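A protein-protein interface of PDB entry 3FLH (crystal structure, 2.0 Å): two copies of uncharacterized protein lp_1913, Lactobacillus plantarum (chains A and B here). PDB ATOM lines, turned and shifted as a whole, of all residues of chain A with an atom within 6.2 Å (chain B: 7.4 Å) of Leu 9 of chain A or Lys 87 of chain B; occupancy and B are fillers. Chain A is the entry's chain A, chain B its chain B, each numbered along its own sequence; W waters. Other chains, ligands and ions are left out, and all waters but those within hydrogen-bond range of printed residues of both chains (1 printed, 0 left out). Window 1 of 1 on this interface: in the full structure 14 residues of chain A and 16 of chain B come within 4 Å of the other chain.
2 positions are printed for both chains. Of the 16 pairs that touch across the chains among the printed residues, none has its exchanged pair printed and touching as well.
Hydrophobic or aromatic side chains of chain A that line the printed part of chain B: Ile 6, Leu 8, Leu 9, Tyr 12 and Leu 13. Of the 21 printed residues of chain B, 8 touch a printed residue of chain A. Printed residues of chain B that touch a printed residue of chain A: Thr 11, Tyr 12, Leu 15, Thr 84, Lys 87, Thr 88, Leu 91 and Leu 94. Hydrophobic or aromatic side chains of chain B within 4 Å of the printed part of chain A: Leu 15, Leu 91 and Leu 94. Among the printed residues, 16 pairs touch across the chains. Among the printed residues, no Asp or Glu carboxylate lies within 4 Å of a Lys or Arg side-chain nitrogen of the other chain.
The backbone carbonyl oxygen (O) of Ile 6 of chain A is in hydrogen-bond range of the side-chain hydroxyl (OG1) of Thr 10 of chain A (2.9 Å). The side-chain hydroxyl (OH) of Tyr 12 of chain B lies within hydrogen-bond range of the side-chain hydroxyl (OH) of Tyr 16 of chain B (3.0 Å). O of Leu 15 of chain B sits at hydrogen-bond distance from N of Glu 102 of chain B (2.8 Å). OH of Tyr 16 of chain B is in hydrogen-bond range of NZ of Lys 87 of chain B, 3.2 Å away. OG1 of Thr 88 of chain B sits at hydrogen-bond distance from O of Thr 84 of chain B (3.1 Å). The backbone carbonyl oxygen (O) of Leu 91 of chain B lies within hydrogen-bond range of the side-chain hydroxyl (OG) of Ser 95 of chain B, at 2.7 Å.
Leu 9 of chain A touches just these residues of chain B: Leu 15, Lys 87, Leu 91 and Leu 94. Of the printed residues of chain B, Leu 13 of chain A touches Thr 84 (3.9 Å), Thr 88 (3.5 Å) and Leu 91 (3.9 Å). Of the printed residues of chain A, Leu 15 of chain B touches Lys 5 (3.7 Å) and Leu 9 (3.9 Å). Of the printed residues of chain A, Thr 84 of chain B touches Leu 13. Leu 85 of chain B touches none of the printed residues of chain A. Gly 86 of chain B touches none of the printed residues of chain A. Of chain A, only Leu 9 and Tyr 12 come within 4 Å of Lys 87 of chain B. Of the printed residues of chain A, Leu 94 of chain B touches Lys 5, Ile 6 and Leu 9.
Lys 4 of chain A touches Thr 11 of chain B (O to CG2, 3.8 Å). Lys 5 of chain A touches Leu 15 of chain B (CB to CD2, 3.7 Å). Lys 5 of chain A touches Leu 94 of chain B (CB to CD1, 3.9 Å). CD1 of Leu 91 of chain B touches CG2 of Ile 6 of chain A, 3.9 Å away. Leu 9 of chain A touches Leu 15 of chain B. Leu 91 of chain B touches Leu 9 of chain A. Thr 10 of chain A touches Leu 91 of chain B. Lys 87 of chain B touches Tyr 12 of chain A (CE to CE2, 3.4 Å). Thr 84 of chain B touches Leu 13 of chain A (CB to CD2, 3.9 Å). Leu 13 of chain A touches Leu 91 of chain B.
Water W1 lies within hydrogen-bond range of the side-chain hydroxyl (OH) of Tyr 12 of chain A and the side-chain hydroxyl (OH) of Tyr 12 of chain B.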
ATOM      1  N   LYS A   4      26.108 -26.294  -6.464  1.00  0.00           N
ATOM      2  CA  LYS A   4      26.687 -24.962  -6.581  1.00  0.00           C
ATOM      3  C   LYS A   4      27.056 -24.618  -8.017  1.00  0.00           C
ATOM      4  O   LYS A   4      26.801 -23.508  -8.483  1.00  0.00           O
ATOM      5  CB  LYS A   4      27.921 -24.807  -5.689  1.00  0.00           C
ATOM      6  CG  LYS A   4      27.589 -24.504  -4.244  1.00  0.00           C
ATOM      7  CD  LYS A   4      28.807 -24.013  -3.485  1.00  0.00           C
ATOM      8  CE  LYS A   4      28.397 -23.422  -2.142  1.00  0.00           C
ATOM      9  NZ  LYS A   4      27.475 -22.255  -2.323  1.00  0.00           N
ATOM     10  N   LYS A   5      27.656 -25.569  -8.719  1.00  0.00           N
ATOM     11  CA  LYS A   5      28.047 -25.341 -10.106  1.00  0.00           C
ATOM     12  C   LYS A   5      26.835 -25.037 -10.991  1.00  0.00           C
ATOM     13  O   LYS A   5      26.855 -24.089 -11.775  1.00  0.00           O
ATOM     14  CB  LYS A   5      28.773 -26.561 -10.673  1.00  0.00           C
ATOM     15  CG  LYS A   5      30.133 -26.831 -10.079  1.00  0.00           C
ATOM     16  CD  LYS A   5      30.706 -28.092 -10.699  1.00  0.00           C
ATOM     17  CE  LYS A   5      32.020 -28.482 -10.066  1.00  0.00           C
ATOM     18  NZ  LYS A   5      32.576 -29.690 -10.743  1.00  0.00           N
ATOM     19  N   ILE A   6      25.791 -25.851 -10.859  1.00  0.00           N
ATOM     20  CA  ILE A   6      24.566 -25.689 -11.641  1.00  0.00           C
ATOM     21  C   ILE A   6      23.918 -24.321 -11.382  1.00  0.00           C
ATOM     22  O   ILE A   6      23.471 -23.648 -12.310  1.00  0.00           O
ATOM     23  CB  ILE A   6      23.563 -26.852 -11.322  1.00  0.00           C
ATOM     24  CG1 ILE A   6      24.162 -28.184 -11.800  1.00  0.00           C
ATOM     25  CG2 ILE A   6      22.225 -26.619 -12.017  1.00  0.00           C
ATOM     26  CD1 ILE A   6      23.355 -29.433 -11.429  1.00  0.00           C
ATOM     27  N   GLU A   7      23.886 -23.918 -10.117  1.00  0.00           N
ATOM     28  CA  GLU A   7      23.325 -22.636  -9.726  1.00  0.00           C
ATOM     29  C   GLU A   7      24.072 -21.486 -10.415  1.00  0.00           C
ATOM     30  O   GLU A   7      23.453 -20.588 -10.992  1.00  0.00           O
ATOM     31  CB  GLU A   7      23.426 -22.476  -8.206  1.00  0.00           C
ATOM     32  CG  GLU A   7      22.795 -21.210  -7.668  1.00  0.00           C
ATOM     33  CD  GLU A   7      21.289 -21.224  -7.820  1.00  0.00           C
ATOM     34  OE1 GLU A   7      20.641 -22.131  -7.240  1.00  0.00           O
ATOM     35  OE2 GLU A   7      20.756 -20.337  -8.526  1.00  0.00           O
ATOM     36  N   LEU A   8      25.400 -21.514 -10.350  1.00  0.00           N
ATOM     37  CA  LEU A   8      26.203 -20.464 -10.970  1.00  0.00           C
ATOM     38  C   LEU A   8      26.035 -20.488 -12.487  1.00  0.00           C
ATOM     39  O   LEU A   8      25.823 -19.447 -13.102  1.00  0.00           O
ATOM     40  CB  LEU A   8      27.682 -20.629 -10.613  1.00  0.00           C
ATOM     41  CG  LEU A   8      28.687 -19.715 -11.333  1.00  0.00           C
ATOM     42  CD1 LEU A   8      28.449 -18.233 -10.952  1.00  0.00           C
ATOM     43  CD2 LEU A   8      30.090 -20.136 -10.945  1.00  0.00           C
ATOM     44  N   LEU A   9      26.121 -21.674 -13.088  1.00  0.00           N
ATOM     45  CA  LEU A   9      25.970 -21.791 -14.532  1.00  0.00           C
ATOM     46  C   LEU A   9      24.625 -21.242 -14.997  1.00  0.00           C
ATOM     47  O   LEU A   9      24.536 -20.555 -16.015  1.00  0.00           O
ATOM     48  CB  LEU A   9      26.101 -23.251 -14.968  1.00  0.00           C
ATOM     49  CG  LEU A   9      27.509 -23.848 -14.976  1.00  0.00           C
ATOM     50  CD1 LEU A   9      27.405 -25.364 -15.113  1.00  0.00           C
ATOM     51  CD2 LEU A   9      28.326 -23.257 -16.140  1.00  0.00           C
ATOM     52  N   THR A  10      23.572 -21.540 -14.253  1.00  0.00           N
ATOM     53  CA  THR A  10      22.247 -21.067 -14.636  1.00  0.00           C
ATOM     54  C   THR A  10      22.147 -19.545 -14.527  1.00  0.00           C
ATOM     55  O   THR A  10      21.655 -18.892 -15.441  1.00  0.00           O
ATOM     56  CB  THR A  10      21.165 -21.734 -13.775  1.00  0.00           C
ATOM     57  OG1 THR A  10      21.219 -23.148 -13.984  1.00  0.00           O
ATOM     58  CG2 THR A  10      19.783 -21.232 -14.155  1.00  0.00           C
ATOM     59  N   THR A  11      22.618 -18.978 -13.418  1.00  0.00           N
ATOM     60  CA  THR A  11      22.566 -17.529 -13.260  1.00  0.00           C
ATOM     61  C   THR A  11      23.474 -16.859 -14.295  1.00  0.00           C
ATOM     62  O   THR A  11      23.095 -15.867 -14.932  1.00  0.00           O
ATOM     63  CB  THR A  11      23.009 -17.093 -11.850  1.00  0.00           C
ATOM     64  OG1 THR A  11      22.103 -17.632 -10.882  1.00  0.00           O
ATOM     65  CG2 THR A  11      23.006 -15.562 -11.734  1.00  0.00           C
ATOM     66  N   TYR A  12      24.666 -17.418 -14.465  1.00  0.00           N
ATOM     67  CA  TYR A  12      25.637 -16.895 -15.412  1.00  0.00           C
ATOM     68  C   TYR A  12      25.070 -16.849 -16.824  1.00  0.00           C
ATOM     69  O   TYR A  12      25.119 -15.812 -17.493  1.00  0.00           O
ATOM     70  CB  TYR A  12      26.902 -17.760 -15.421  1.00  0.00           C
ATOM     71  CG  TYR A  12      28.073 -17.107 -16.127  1.00  0.00           C
ATOM     72  CD1 TYR A  12      28.912 -16.221 -15.447  1.00  0.00           C
ATOM     73  CD2 TYR A  12      28.335 -17.368 -17.470  1.00  0.00           C
ATOM     74  CE1 TYR A  12      29.985 -15.614 -16.085  1.00  0.00           C
ATOM     75  CE2 TYR A  12      29.404 -16.765 -18.122  1.00  0.00           C
ATOM     76  CZ  TYR A  12      30.227 -15.891 -17.423  1.00  0.00           C
ATOM     77  OH  TYR A  12      31.290 -15.298 -18.052  1.00  0.00           O
ATOM     78  N   LEU A  13      24.536 -17.976 -17.285  1.00  0.00           N
ATOM     79  CA  LEU A  13      23.977 -18.032 -18.633  1.00  0.00           C
ATOM     80  C   LEU A  13      22.769 -17.116 -18.833  1.00  0.00           C
ATOM     81  O   LEU A  13      22.553 -16.612 -19.938  1.00  0.00           O
ATOM     82  CB  LEU A  13      23.622 -19.478 -18.996  1.00  0.00           C
ATOM     83  CG  LEU A  13      24.868 -20.348 -19.242  1.00  0.00           C
ATOM     84  CD1 LEU A  13      24.471 -21.824 -19.336  1.00  0.00           C
ATOM     85  CD2 LEU A  13      25.560 -19.891 -20.534  1.00  0.00           C
ATOM     86  N   SER A  14      21.993 -16.885 -17.774  1.00  0.00           N
ATOM     87  CA  SER A  14      20.825 -16.008 -17.887  1.00  0.00           C
ATOM     88  C   SER A  14      21.200 -14.551 -18.198  1.00  0.00           C
ATOM     89  O   SER A  14      20.333 -13.724 -18.484  1.00  0.00           O
ATOM     90  CB  SER A  14      19.984 -16.051 -16.607  1.00  0.00           C
ATOM     91  OG  SER A  14      20.634 -15.402 -15.529  1.00  0.00           O
ATOM     92  N   THR B  11      33.919 -21.623  -6.965  1.00  0.00           N
ATOM     93  CA  THR B  11      32.885 -22.285  -7.756  1.00  0.00           C
ATOM     94  C   THR B  11      33.120 -22.121  -9.253  1.00  0.00           C
ATOM     95  O   THR B  11      32.922 -23.063 -10.026  1.00  0.00           O
ATOM     96  CB  THR B  11      31.487 -21.741  -7.416  1.00  0.00           C
ATOM     97  OG1 THR B  11      31.250 -21.883  -6.008  1.00  0.00           O
ATOM     98  CG2 THR B  11      30.417 -22.518  -8.180  1.00  0.00           C
ATOM     99  N   TYR B  12      33.542 -20.926  -9.661  1.00  0.00           N
ATOM    100  CA  TYR B  12      33.786 -20.654 -11.081  1.00  0.00           C
ATOM    101  C   TYR B  12      34.942 -21.521 -11.601  1.00  0.00           C
ATOM    102  O   TYR B  12      34.861 -22.085 -12.694  1.00  0.00           O
ATOM    103  CB  TYR B  12      34.109 -19.167 -11.292  1.00  0.00           C
ATOM    104  CG  TYR B  12      34.239 -18.756 -12.751  1.00  0.00           C
ATOM    105  CD1 TYR B  12      33.128 -18.327 -13.477  1.00  0.00           C
ATOM    106  CD2 TYR B  12      35.467 -18.812 -13.404  1.00  0.00           C
ATOM    107  CE1 TYR B  12      33.236 -17.965 -14.822  1.00  0.00           C
ATOM    108  CE2 TYR B  12      35.588 -18.454 -14.751  1.00  0.00           C
ATOM    109  CZ  TYR B  12      34.473 -18.034 -15.451  1.00  0.00           C
ATOM    110  OH  TYR B  12      34.580 -17.698 -16.784  1.00  0.00           O
ATOM    111  N   LEU B  15      34.541 -25.265 -12.443  1.00  0.00           N
ATOM    112  CA  LEU B  15      33.885 -25.577 -13.710  1.00  0.00           C
ATOM    113  C   LEU B  15      34.903 -25.954 -14.776  1.00  0.00           C
ATOM    114  O   LEU B  15      34.556 -26.580 -15.778  1.00  0.00           O
ATOM    115  CB  LEU B  15      33.089 -24.368 -14.207  1.00  0.00           C
ATOM    116  CG  LEU B  15      31.970 -23.824 -13.320  1.00  0.00           C
ATOM    117  CD1 LEU B  15      31.465 -22.523 -13.913  1.00  0.00           C
ATOM    118  CD2 LEU B  15      30.842 -24.853 -13.204  1.00  0.00           C
ATOM    119  N   TYR B  16      36.160 -25.579 -14.555  1.00  0.00           N
ATOM    120  CA  TYR B  16      37.212 -25.845 -15.529  1.00  0.00           C
ATOM    121  C   TYR B  16      38.219 -26.920 -15.151  1.00  0.00           C
ATOM    122  O   TYR B  16      38.359 -27.292 -13.985  1.00  0.00           O
ATOM    123  CB  TYR B  16      37.999 -24.562 -15.829  1.00  0.00           C
ATOM    124  CG  TYR B  16      37.211 -23.447 -16.475  1.00  0.00           C
ATOM    125  CD1 TYR B  16      36.391 -22.613 -15.715  1.00  0.00           C
ATOM    126  CD2 TYR B  16      37.308 -23.207 -17.846  1.00  0.00           C
ATOM    127  CE1 TYR B  16      35.691 -21.561 -16.306  1.00  0.00           C
ATOM    128  CE2 TYR B  16      36.612 -22.159 -18.449  1.00  0.00           C
ATOM    129  CZ  TYR B  16      35.806 -21.339 -17.672  1.00  0.00           C
ATOM    130  OH  TYR B  16      35.115 -20.299 -18.258  1.00  0.00           O
ATOM    131  N   VAL B  38      32.445 -29.414 -28.846  1.00  0.00           N
ATOM    132  CA  VAL B  38      31.073 -28.935 -28.998  1.00  0.00           C
ATOM    133  C   VAL B  38      30.891 -27.790 -29.989  1.00  0.00           C
ATOM    134  O   VAL B  38      29.860 -27.118 -29.975  1.00  0.00           O
ATOM    135  CB  VAL B  38      30.478 -28.509 -27.638  1.00  0.00           C
ATOM    136  CG1 VAL B  38      30.563 -29.670 -26.651  1.00  0.00           C
ATOM    137  CG2 VAL B  38      31.220 -27.300 -27.095  1.00  0.00           C
ATOM    138  N   VAL B  76      34.514 -30.459 -22.224  1.00  0.00           N
ATOM    139  CA  VAL B  76      33.976 -29.822 -23.418  1.00  0.00           C
ATOM    140  C   VAL B  76      34.798 -28.597 -23.815  1.00  0.00           C
ATOM    141  O   VAL B  76      35.494 -28.021 -22.985  1.00  0.00           O
ATOM    142  CB  VAL B  76      32.506 -29.370 -23.193  1.00  0.00           C
ATOM    143  CG1 VAL B  76      31.634 -30.562 -22.840  1.00  0.00           C
ATOM    144  CG2 VAL B  76      32.451 -28.335 -22.082  1.00  0.00           C
ATOM    145  N   GLY B  81      37.477 -19.638 -25.580  1.00  0.00           N
ATOM    146  CA  GLY B  81      36.863 -19.594 -24.266  1.00  0.00           C
ATOM    147  C   GLY B  81      35.845 -18.483 -24.088  1.00  0.00           C
ATOM    148  O   GLY B  81      34.997 -18.555 -23.202  1.00  0.00           O
ATOM    149  N   THR B  83      33.184 -17.715 -25.692  1.00  0.00           N
ATOM    150  CA  THR B  83      31.785 -18.035 -25.959  1.00  0.00           C
ATOM    151  C   THR B  83      31.129 -18.641 -24.731  1.00  0.00           C
ATOM    152  O   THR B  83      31.771 -18.830 -23.702  1.00  0.00           O
ATOM    153  CB  THR B  83      31.630 -19.036 -27.145  1.00  0.00           C
ATOM    154  OG1 THR B  83      32.084 -20.337 -26.746  1.00  0.00           O
ATOM    155  CG2 THR B  83      32.439 -18.573 -28.353  1.00  0.00           C
ATOM    156  N   THR B  84      29.844 -18.942 -24.845  1.00  0.00           N
ATOM    157  CA  THR B  84      29.092 -19.540 -23.750  1.00  0.00           C
ATOM    158  C   THR B  84      28.734 -20.982 -24.072  1.00  0.00           C
ATOM    159  O   THR B  84      28.066 -21.642 -23.280  1.00  0.00           O
ATOM    160  CB  THR B  84      27.769 -18.775 -23.507  1.00  0.00           C
ATOM    161  OG1 THR B  84      27.024 -18.719 -24.734  1.00  0.00           O
ATOM    162  CG2 THR B  84      28.050 -17.351 -23.020  1.00  0.00           C
ATOM    163  N   LEU B  85      29.156 -21.468 -25.237  1.00  0.00           N
ATOM    164  CA  LEU B  85      28.835 -22.842 -25.649  1.00  0.00           C
ATOM    165  C   LEU B  85      29.384 -23.886 -24.689  1.00  0.00           C
ATOM    166  O   LEU B  85      28.772 -24.934 -24.496  1.00  0.00           O
ATOM    167  CB  LEU B  85      29.370 -23.132 -27.059  1.00  0.00           C
ATOM    168  CG  LEU B  85      28.626 -22.567 -28.274  1.00  0.00           C
ATOM    169  CD1 LEU B  85      27.234 -23.198 -28.388  1.00  0.00           C
ATOM    170  CD2 LEU B  85      28.521 -21.064 -28.124  1.00  0.00           C
ATOM    171  N   GLY B  86      30.543 -23.604 -24.107  1.00  0.00           N
ATOM    172  CA  GLY B  86      31.138 -24.542 -23.173  1.00  0.00           C
ATOM    173  C   GLY B  86      30.320 -24.663 -21.902  1.00  0.00           C
ATOM    174  O   GLY B  86      30.084 -25.765 -21.405  1.00  0.00           O
ATOM    175  N   LYS B  87      29.872 -23.528 -21.374  1.00  0.00           N
ATOM    176  CA  LYS B  87      29.085 -23.543 -20.149  1.00  0.00           C
ATOM    177  C   LYS B  87      27.703 -24.137 -20.379  1.00  0.00           C
ATOM    178  O   LYS B  87      27.170 -24.839 -19.518  1.00  0.00           O
ATOM    179  CB  LYS B  87      28.973 -22.127 -19.572  1.00  0.00           C
ATOM    180  CG  LYS B  87      30.300 -21.558 -19.062  1.00  0.00           C
ATOM    181  CD  LYS B  87      30.113 -20.141 -18.533  1.00  0.00           C
ATOM    182  CE  LYS B  87      31.433 -19.485 -18.127  1.00  0.00           C
ATOM    183  NZ  LYS B  87      32.122 -20.197 -17.027  1.00  0.00           N
ATOM    184  N   THR B  88      27.122 -23.865 -21.541  1.00  0.00           N
ATOM    185  CA  THR B  88      25.810 -24.404 -21.852  1.00  0.00           C
ATOM    186  C   THR B  88      25.892 -25.931 -21.935  1.00  0.00           C
ATOM    187  O   THR B  88      25.034 -26.633 -21.401  1.00  0.00           O
ATOM    188  CB  THR B  88      25.276 -23.782 -23.163  1.00  0.00           C
ATOM    189  OG1 THR B  88      25.053 -22.383 -22.942  1.00  0.00           O
ATOM    190  CG2 THR B  88      23.968 -24.427 -23.585  1.00  0.00           C
ATOM    191  N   ALA B  89      26.932 -26.443 -22.582  1.00  0.00           N
ATOM    192  CA  ALA B  89      27.114 -27.891 -22.678  1.00  0.00           C
ATOM    193  C   ALA B  89      27.354 -28.440 -21.269  1.00  0.00           C
ATOM    194  O   ALA B  89      26.776 -29.454 -20.886  1.00  0.00           O
ATOM    195  CB  ALA B  89      28.312 -28.219 -23.574  1.00  0.00           C
ATOM    196  N   LEU B  90      28.210 -27.762 -20.502  1.00  0.00           N
ATOM    197  CA  LEU B  90      28.514 -28.196 -19.145  1.00  0.00           C
ATOM    198  C   LEU B  90      27.243 -28.307 -18.309  1.00  0.00           C
ATOM    199  O   LEU B  90      27.068 -29.276 -17.569  1.00  0.00           O
ATOM    200  CB  LEU B  90      29.500 -27.231 -18.467  1.00  0.00           C
ATOM    201  CG  LEU B  90      30.064 -27.659 -17.101  1.00  0.00           C
ATOM    202  CD1 LEU B  90      30.819 -28.990 -17.241  1.00  0.00           C
ATOM    203  CD2 LEU B  90      31.006 -26.589 -16.558  1.00  0.00           C
ATOM    204  N   LEU B  91      26.354 -27.324 -18.430  1.00  0.00           N
ATOM    205  CA  LEU B  91      25.104 -27.325 -17.669  1.00  0.00           C
ATOM    206  C   LEU B  91      24.244 -28.540 -18.003  1.00  0.00           C
ATOM    207  O   LEU B  91      23.611 -29.136 -17.124  1.00  0.00           O
ATOM    208  CB  LEU B  91      24.313 -26.039 -17.942  1.00  0.00           C
ATOM    209  CG  LEU B  91      22.974 -25.904 -17.209  1.00  0.00           C
ATOM    210  CD1 LEU B  91      23.179 -26.084 -15.716  1.00  0.00           C
ATOM    211  CD2 LEU B  91      22.364 -24.535 -17.502  1.00  0.00           C
ATOM    212  N   VAL B  92      24.221 -28.903 -19.279  1.00  0.00           N
ATOM    213  CA  VAL B  92      23.454 -30.056 -19.731  1.00  0.00           C
ATOM    214  C   VAL B  92      24.017 -31.334 -19.107  1.00  0.00           C
ATOM    215  O   VAL B  92      23.268 -32.158 -18.572  1.00  0.00           O
ATOM    216  CB  VAL B  92      23.494 -30.167 -21.278  1.00  0.00           C
ATOM    217  CG1 VAL B  92      22.797 -31.439 -21.739  1.00  0.00           C
ATOM    218  CG2 VAL B  92      22.822 -28.948 -21.895  1.00  0.00           C
ATOM    219  N   LEU B  93      25.338 -31.485 -19.162  1.00  0.00           N
ATOM    220  CA  LEU B  93      26.004 -32.665 -18.616  1.00  0.00           C
ATOM    221  C   LEU B  93      25.830 -32.780 -17.098  1.00  0.00           C
ATOM    222  O   LEU B  93      25.436 -33.832 -16.586  1.00  0.00           O
ATOM    223  CB  LEU B  93      27.498 -32.640 -18.979  1.00  0.00           C
ATOM    224  CG  LEU B  93      27.850 -32.811 -20.458  1.00  0.00           C
ATOM    225  CD1 LEU B  93      29.285 -32.375 -20.721  1.00  0.00           C
ATOM    226  CD2 LEU B  93      27.649 -34.279 -20.854  1.00  0.00           C
ATOM    227  N   LEU B  94      26.126 -31.700 -16.384  1.00  0.00           N
ATOM    228  CA  LEU B  94      25.992 -31.701 -14.929  1.00  0.00           C
ATOM    229  C   LEU B  94      24.530 -31.902 -14.503  1.00  0.00           C
ATOM    230  O   LEU B  94      24.262 -32.580 -13.513  1.00  0.00           O
ATOM    231  CB  LEU B  94      26.550 -30.397 -14.334  1.00  0.00           C
ATOM    232  CG  LEU B  94      28.026 -30.020 -14.598  1.00  0.00           C
ATOM    233  CD1 LEU B  94      28.340 -28.709 -13.864  1.00  0.00           C
ATOM    234  CD2 LEU B  94      28.964 -31.123 -14.119  1.00  0.00           C
ATOM    235  N   SER B  95      23.582 -31.329 -15.244  1.00  0.00           N
ATOM    236  CA  SER B  95      22.164 -31.497 -14.897  1.00  0.00           C
ATOM    237  C   SER B  95      21.717 -32.943 -15.101  1.00  0.00           C
ATOM    238  O   SER B  95      20.791 -33.412 -14.439  1.00  0.00           O
ATOM    239  CB  SER B  95      21.275 -30.582 -15.746  1.00  0.00           C
ATOM    240  OG  SER B  95      21.492 -29.216 -15.434  1.00  0.00           O
ATOM    241  N   GLU B 102      34.883 -27.749 -18.341  1.00  0.00           N
ATOM    242  CA  GLU B 102      35.151 -27.063 -19.589  1.00  0.00           C
ATOM    243  C   GLU B 102      36.681 -26.991 -19.675  1.00  0.00           C
ATOM    244  O   GLU B 102      37.342 -26.802 -18.651  1.00  0.00           O
ATOM    245  CB  GLU B 102      34.572 -25.649 -19.573  1.00  0.00           C
ATOM    246  CG  GLU B 102      34.552 -25.045 -20.952  1.00  0.00           C
ATOM    247  CD  GLU B 102      34.026 -23.625 -21.002  1.00  0.00           C
ATOM    248  OE1 GLU B 102      33.005 -23.330 -20.341  1.00  0.00           O
ATOM    249  OE2 GLU B 102      34.637 -22.814 -21.727  1.00  0.00           O
HETATM  250  O   HOH W   1      33.668 -15.107 -17.184  1.00  0.00           O
